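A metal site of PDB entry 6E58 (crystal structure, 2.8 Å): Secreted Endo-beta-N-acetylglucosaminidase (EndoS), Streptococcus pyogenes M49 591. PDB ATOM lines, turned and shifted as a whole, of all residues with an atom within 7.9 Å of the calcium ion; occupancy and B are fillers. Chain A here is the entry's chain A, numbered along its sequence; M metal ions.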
ATOM      1  N   GLN A 654     -30.586 -21.936  -5.102  1.00  0.00           N
ATOM      2  CA  GLN A 654     -29.754 -21.915  -3.900  1.00  0.00           C
ATOM      3  C   GLN A 654     -28.607 -20.901  -4.040  1.00  0.00           C
ATOM      4  O   GLN A 654     -28.210 -20.277  -3.038  1.00  0.00           O
ATOM      5  CB  GLN A 654     -29.225 -23.304  -3.595  1.00  0.00           C
ATOM      6  CG  GLN A 654     -30.304 -24.293  -3.119  1.00  0.00           C
ATOM      7  CD  GLN A 654     -30.813 -23.983  -1.705  1.00  0.00           C
ATOM      8  OE1 GLN A 654     -32.020 -24.016  -1.454  1.00  0.00           O
ATOM      9  NE2 GLN A 654     -29.885 -23.676  -0.785  1.00  0.00           N
ATOM     10  N   ALA A 655     -28.086 -20.702  -5.246  1.00  0.00           N
ATOM     11  CA  ALA A 655     -26.902 -19.849  -5.389  1.00  0.00           C
ATOM     12  C   ALA A 655     -27.224 -18.394  -5.048  1.00  0.00           C
ATOM     13  O   ALA A 655     -26.419 -17.718  -4.411  1.00  0.00           O
ATOM     14  CB  ALA A 655     -26.355 -19.927  -6.806  1.00  0.00           C
ATOM     15  N   LYS A 656     -28.385 -17.911  -5.462  1.00  0.00           N
ATOM     16  CA  LYS A 656     -28.659 -16.499  -5.248  1.00  0.00           C
ATOM     17  C   LYS A 656     -28.779 -16.151  -3.765  1.00  0.00           C
ATOM     18  O   LYS A 656     -28.747 -14.963  -3.409  1.00  0.00           O
ATOM     19  CB  LYS A 656     -29.881 -16.046  -6.028  1.00  0.00           C
ATOM     20  CG  LYS A 656     -31.103 -16.877  -5.927  1.00  0.00           C
ATOM     21  CD  LYS A 656     -32.219 -16.113  -6.614  1.00  0.00           C
ATOM     22  CE  LYS A 656     -32.033 -16.106  -8.117  1.00  0.00           C
ATOM     23  NZ  LYS A 656     -32.704 -17.313  -8.672  1.00  0.00           N
ATOM     24  N   LYS A 657     -28.910 -17.135  -2.891  1.00  0.00           N
ATOM     25  CA  LYS A 657     -29.043 -16.839  -1.482  1.00  0.00           C
ATOM     26  C   LYS A 657     -27.700 -16.598  -0.792  1.00  0.00           C
ATOM     27  O   LYS A 657     -27.689 -16.473   0.436  1.00  0.00           O
ATOM     28  CB  LYS A 657     -29.810 -17.938  -0.757  1.00  0.00           C
ATOM     29  CG  LYS A 657     -31.287 -17.939  -1.055  1.00  0.00           C
ATOM     30  CD  LYS A 657     -31.971 -19.004  -0.232  1.00  0.00           C
ATOM     31  CE  LYS A 657     -31.316 -20.363  -0.412  1.00  0.00           C
ATOM     32  NZ  LYS A 657     -32.340 -21.439  -0.311  1.00  0.00           N
ATOM     33  N   ILE A 658     -26.588 -16.542  -1.522  1.00  0.00           N
ATOM     34  CA  ILE A 658     -25.341 -16.094  -0.917  1.00  0.00           C
ATOM     35  C   ILE A 658     -25.098 -14.603  -1.146  1.00  0.00           C
ATOM     36  O   ILE A 658     -24.038 -14.085  -0.799  1.00  0.00           O
ATOM     37  CB  ILE A 658     -24.160 -16.946  -1.402  1.00  0.00           C
ATOM     38  CG1 ILE A 658     -23.718 -16.553  -2.788  1.00  0.00           C
ATOM     39  CG2 ILE A 658     -24.528 -18.402  -1.394  1.00  0.00           C
ATOM     40  CD1 ILE A 658     -22.397 -17.112  -3.117  1.00  0.00           C
ATOM     41  N   PHE A 659     -26.075 -13.908  -1.726  1.00  0.00           N
ATOM     42  CA  PHE A 659     -25.975 -12.484  -2.002  1.00  0.00           C
ATOM     43  C   PHE A 659     -27.158 -11.699  -1.456  1.00  0.00           C
ATOM     44  O   PHE A 659     -27.405 -10.562  -1.891  1.00  0.00           O
ATOM     45  CB  PHE A 659     -25.853 -12.276  -3.508  1.00  0.00           C
ATOM     46  CG  PHE A 659     -24.638 -12.906  -4.105  1.00  0.00           C
ATOM     47  CD1 PHE A 659     -23.373 -12.577  -3.640  1.00  0.00           C
ATOM     48  CD2 PHE A 659     -24.754 -13.871  -5.106  1.00  0.00           C
ATOM     49  CE1 PHE A 659     -22.247 -13.153  -4.175  1.00  0.00           C
ATOM     50  CE2 PHE A 659     -23.641 -14.452  -5.647  1.00  0.00           C
ATOM     51  CZ  PHE A 659     -22.382 -14.095  -5.172  1.00  0.00           C
ATOM     52  N   ASP A 660     -27.892 -12.266  -0.495  1.00  0.00           N
ATOM     53  CA  ASP A 660     -28.908 -11.518   0.236  1.00  0.00           C
ATOM     54  C   ASP A 660     -28.247 -10.918   1.488  1.00  0.00           C
ATOM     55  O   ASP A 660     -27.034 -10.695   1.523  1.00  0.00           O
ATOM     56  CB  ASP A 660     -30.111 -12.414   0.531  1.00  0.00           C
ATOM     57  CG  ASP A 660     -29.752 -13.657   1.328  1.00  0.00           C
ATOM     58  OD1 ASP A 660     -28.681 -13.662   1.986  1.00  0.00           O
ATOM     59  OD2 ASP A 660     -30.548 -14.638   1.334  1.00  0.00           O
ATOM     60  N   GLY A 661     -29.028 -10.605   2.508  1.00  0.00           N
ATOM     61  CA  GLY A 661     -28.419  -9.988   3.662  1.00  0.00           C
ATOM     62  C   GLY A 661     -27.982 -10.992   4.708  1.00  0.00           C
ATOM     63  O   GLY A 661     -27.098 -10.719   5.518  1.00  0.00           O
ATOM     64  N   GLU A 662     -28.620 -12.149   4.690  1.00  0.00           N
ATOM     65  CA  GLU A 662     -28.683 -13.028   5.834  1.00  0.00           C
ATOM     66  C   GLU A 662     -27.625 -14.135   5.773  1.00  0.00           C
ATOM     67  O   GLU A 662     -26.880 -14.262   4.809  1.00  0.00           O
ATOM     68  CB  GLU A 662     -30.089 -13.633   5.925  1.00  0.00           C
ATOM     69  CG  GLU A 662     -31.205 -12.579   5.776  1.00  0.00           C
ATOM     70  CD  GLU A 662     -32.325 -12.728   6.817  1.00  0.00           C
ATOM     71  OE1 GLU A 662     -32.417 -11.850   7.716  1.00  0.00           O
ATOM     72  OE2 GLU A 662     -33.100 -13.712   6.726  1.00  0.00           O
ATOM     73  N   LYS A 663     -27.536 -14.885   6.873  1.00  0.00           N
ATOM     74  CA  LYS A 663     -26.769 -16.118   6.944  1.00  0.00           C
ATOM     75  C   LYS A 663     -27.707 -17.301   7.209  1.00  0.00           C
ATOM     76  O   LYS A 663     -27.317 -18.298   7.811  1.00  0.00           O
ATOM     77  CB  LYS A 663     -25.740 -16.065   8.080  1.00  0.00           C
ATOM     78  CG  LYS A 663     -25.169 -14.709   8.448  1.00  0.00           C
ATOM     79  CD  LYS A 663     -24.198 -14.156   7.461  1.00  0.00           C
ATOM     80  CE  LYS A 663     -23.880 -12.708   7.841  1.00  0.00           C
ATOM     81  NZ  LYS A 663     -23.755 -11.773   6.676  1.00  0.00           N
ATOM     82  N   SER A 664     -28.947 -17.203   6.722  1.00  0.00           N
ATOM     83  CA  SER A 664     -30.035 -18.131   7.060  1.00  0.00           C
ATOM     84  C   SER A 664     -30.266 -19.158   5.965  1.00  0.00           C
ATOM     85  O   SER A 664     -31.416 -19.505   5.660  1.00  0.00           O
ATOM     86  CB  SER A 664     -31.330 -17.356   7.336  1.00  0.00           C
ATOM     87  OG  SER A 664     -31.776 -16.616   6.200  1.00  0.00           O
ATOM     88  N   ASP A 665     -29.200 -19.665   5.380  1.00  0.00           N
ATOM     89  CA  ASP A 665     -29.270 -20.442   4.141  1.00  0.00           C
ATOM     90  C   ASP A 665     -27.903 -21.049   3.930  1.00  0.00           C
ATOM     91  O   ASP A 665     -26.953 -20.771   4.679  1.00  0.00           O
ATOM     92  CB  ASP A 665     -29.658 -19.563   2.962  1.00  0.00           C
ATOM     93  CG  ASP A 665     -28.877 -18.247   2.933  1.00  0.00           C
ATOM     94  OD1 ASP A 665     -27.644 -18.322   2.676  1.00  0.00           O
ATOM     95  OD2 ASP A 665     -29.471 -17.156   3.176  1.00  0.00           O
ATOM     96  N   ARG A 666     -27.807 -21.896   2.924  1.00  0.00           N
ATOM     97  CA  ARG A 666     -26.541 -22.560   2.712  1.00  0.00           C
ATOM     98  C   ARG A 666     -26.483 -22.964   1.250  1.00  0.00           C
ATOM     99  O   ARG A 666     -27.511 -23.286   0.653  1.00  0.00           O
ATOM    100  CB  ARG A 666     -26.409 -23.746   3.658  1.00  0.00           C
ATOM    101  CG  ARG A 666     -27.643 -24.606   3.665  1.00  0.00           C
ATOM    102  CD  ARG A 666     -27.413 -25.853   4.497  1.00  0.00           C
ATOM    103  NE  ARG A 666     -28.565 -26.750   4.517  1.00  0.00           N
ATOM    104  CZ  ARG A 666     -28.636 -27.843   5.273  1.00  0.00           C
ATOM    105  NH1 ARG A 666     -27.640 -28.138   6.081  1.00  0.00           N
ATOM    106  NH2 ARG A 666     -29.720 -28.596   5.243  1.00  0.00           N
ATOM    107  N   PHE A 667     -25.297 -22.891   0.667  1.00  0.00           N
ATOM    108  CA  PHE A 667     -25.044 -23.385  -0.683  1.00  0.00           C
ATOM    109  C   PHE A 667     -23.992 -24.486  -0.628  1.00  0.00           C
ATOM    110  O   PHE A 667     -22.906 -24.270  -0.092  1.00  0.00           O
ATOM    111  CB  PHE A 667     -24.571 -22.267  -1.589  1.00  0.00           C
ATOM    112  CG  PHE A 667     -24.213 -22.719  -2.953  1.00  0.00           C
ATOM    113  CD1 PHE A 667     -22.933 -23.171  -3.224  1.00  0.00           C
ATOM    114  CD2 PHE A 667     -25.152 -22.707  -3.963  1.00  0.00           C
ATOM    115  CE1 PHE A 667     -22.618 -23.596  -4.478  1.00  0.00           C
ATOM    116  CE2 PHE A 667     -24.838 -23.131  -5.216  1.00  0.00           C
ATOM    117  CZ  PHE A 667     -23.569 -23.576  -5.485  1.00  0.00           C
ATOM    118  N   PHE A 692     -18.544 -15.950   4.588  1.00  0.00           N
ATOM    119  CA  PHE A 692     -19.151 -16.504   5.802  1.00  0.00           C
ATOM    120  C   PHE A 692     -19.298 -18.003   5.628  1.00  0.00           C
ATOM    121  O   PHE A 692     -20.131 -18.445   4.826  1.00  0.00           O
ATOM    122  CB  PHE A 692     -20.491 -15.853   6.098  1.00  0.00           C
ATOM    123  CG  PHE A 692     -20.398 -14.412   6.421  1.00  0.00           C
ATOM    124  CD1 PHE A 692     -20.306 -13.984   7.730  1.00  0.00           C
ATOM    125  CD2 PHE A 692     -20.383 -13.466   5.418  1.00  0.00           C
ATOM    126  CE1 PHE A 692     -20.211 -12.661   8.037  1.00  0.00           C
ATOM    127  CE2 PHE A 692     -20.294 -12.127   5.741  1.00  0.00           C
ATOM    128  CZ  PHE A 692     -20.217 -11.737   7.043  1.00  0.00           C
ATOM    129  N   TYR A 781     -21.432 -22.969   2.574  1.00  0.00           N
ATOM    130  CA  TYR A 781     -21.194 -21.599   3.032  1.00  0.00           C
ATOM    131  C   TYR A 781     -22.446 -20.768   2.789  1.00  0.00           C
ATOM    132  O   TYR A 781     -23.305 -21.090   1.963  1.00  0.00           O
ATOM    133  CB  TYR A 781     -19.973 -20.944   2.351  1.00  0.00           C
ATOM    134  CG  TYR A 781     -20.081 -20.714   0.884  1.00  0.00           C
ATOM    135  CD1 TYR A 781     -19.721 -21.704  -0.010  1.00  0.00           C
ATOM    136  CD2 TYR A 781     -20.480 -19.488   0.387  1.00  0.00           C
ATOM    137  CE1 TYR A 781     -19.795 -21.493  -1.376  1.00  0.00           C
ATOM    138  CE2 TYR A 781     -20.543 -19.260  -0.979  1.00  0.00           C
ATOM    139  CZ  TYR A 781     -20.196 -20.276  -1.859  1.00  0.00           C
ATOM    140  OH  TYR A 781     -20.263 -20.069  -3.219  1.00  0.00           O
ATOM    141  N   THR A 782     -22.548 -19.678   3.554  1.00  0.00           N
ATOM    142  CA  THR A 782     -23.816 -18.970   3.627  1.00  0.00           C
ATOM    143  C   THR A 782     -23.816 -17.612   2.939  1.00  0.00           C
ATOM    144  O   THR A 782     -24.870 -17.183   2.474  1.00  0.00           O
ATOM    145  CB  THR A 782     -24.240 -18.802   5.095  1.00  0.00           C
ATOM    146  OG1 THR A 782     -23.430 -17.804   5.713  1.00  0.00           O
ATOM    147  CG2 THR A 782     -24.022 -20.101   5.854  1.00  0.00           C
ATOM    148  N   GLU A 783     -22.691 -16.921   2.857  1.00  0.00           N
ATOM    149  CA  GLU A 783     -22.741 -15.554   2.342  1.00  0.00           C
ATOM    150  C   GLU A 783     -21.368 -15.124   1.834  1.00  0.00           C
ATOM    151  O   GLU A 783     -20.355 -15.492   2.410  1.00  0.00           O
ATOM    152  CB  GLU A 783     -23.260 -14.605   3.439  1.00  0.00           C
ATOM    153  CG  GLU A 783     -23.335 -13.173   3.019  1.00  0.00           C
ATOM    154  CD  GLU A 783     -24.643 -12.806   2.355  1.00  0.00           C
ATOM    155  OE1 GLU A 783     -24.756 -11.656   1.884  1.00  0.00           O
ATOM    156  OE2 GLU A 783     -25.556 -13.661   2.317  1.00  0.00           O
ATOM    157  N   LEU A 784     -21.357 -14.352   0.748  1.00  0.00           N
ATOM    158  CA  LEU A 784     -20.131 -13.885   0.102  1.00  0.00           C
ATOM    159  C   LEU A 784     -20.163 -12.369  -0.067  1.00  0.00           C
ATOM    160  O   LEU A 784     -21.144 -11.809  -0.562  1.00  0.00           O
ATOM    161  CB  LEU A 784     -19.947 -14.559  -1.257  1.00  0.00           C
ATOM    162  CG  LEU A 784     -18.639 -14.399  -2.033  1.00  0.00           C
ATOM    163  CD1 LEU A 784     -17.511 -15.221  -1.488  1.00  0.00           C
ATOM    164  CD2 LEU A 784     -18.940 -14.834  -3.439  1.00  0.00           C
HETATM  165 CA    CA M   1     -27.220 -15.589   2.481  1.00  0.00          CA
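The side-chain amino group (NZ) of Lys 657 lies within hydrogen-bond range of the side-chain amide oxygen (OE1) of Gln 654, at 2.8 Å. The backbone NH (N) of Thr 782 lies within hydrogen-bond range of the backbone carbonyl oxygen (O) of Phe 692. The backbone carbonyl oxygen (O) of Glu 783 lies within hydrogen-bond range of the backbone NH (N) of Phe 692 (2.9 Å). OE2 of Glu 662 sits at hydrogen-bond distance from OG of Ser 664 (3.2 Å). The backbone carbonyl oxygen of Ile 658 lies within hydrogen-bond range of the backbone NH of Leu 784 (3.1 Å).
Merely in contact with the calcium ion: Ile 658 (3.9 Å). Within 4 Å of the calcium ion: Lys 657, Ile 658, Asp 660, Glu 662, Asp 665, Thr 782 and Glu 783. The nearest printed residue that does not touch the calcium ion is Lys 663 (4.5 Å).
The calcium ion is bound by O of Lys 657 (2.3 Å), OD1 of Asp 660 (2.5 Å), OE2 of Glu 783 (2.6 Å), O of Glu 662 (2.7 Å), OD1 of Asp 665 (2.8 Å), OD2 of Asp 665 (2.8 Å) and O of Thr 782 (2.8 Å). The calcium ion has seven donor atoms within binding distance.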
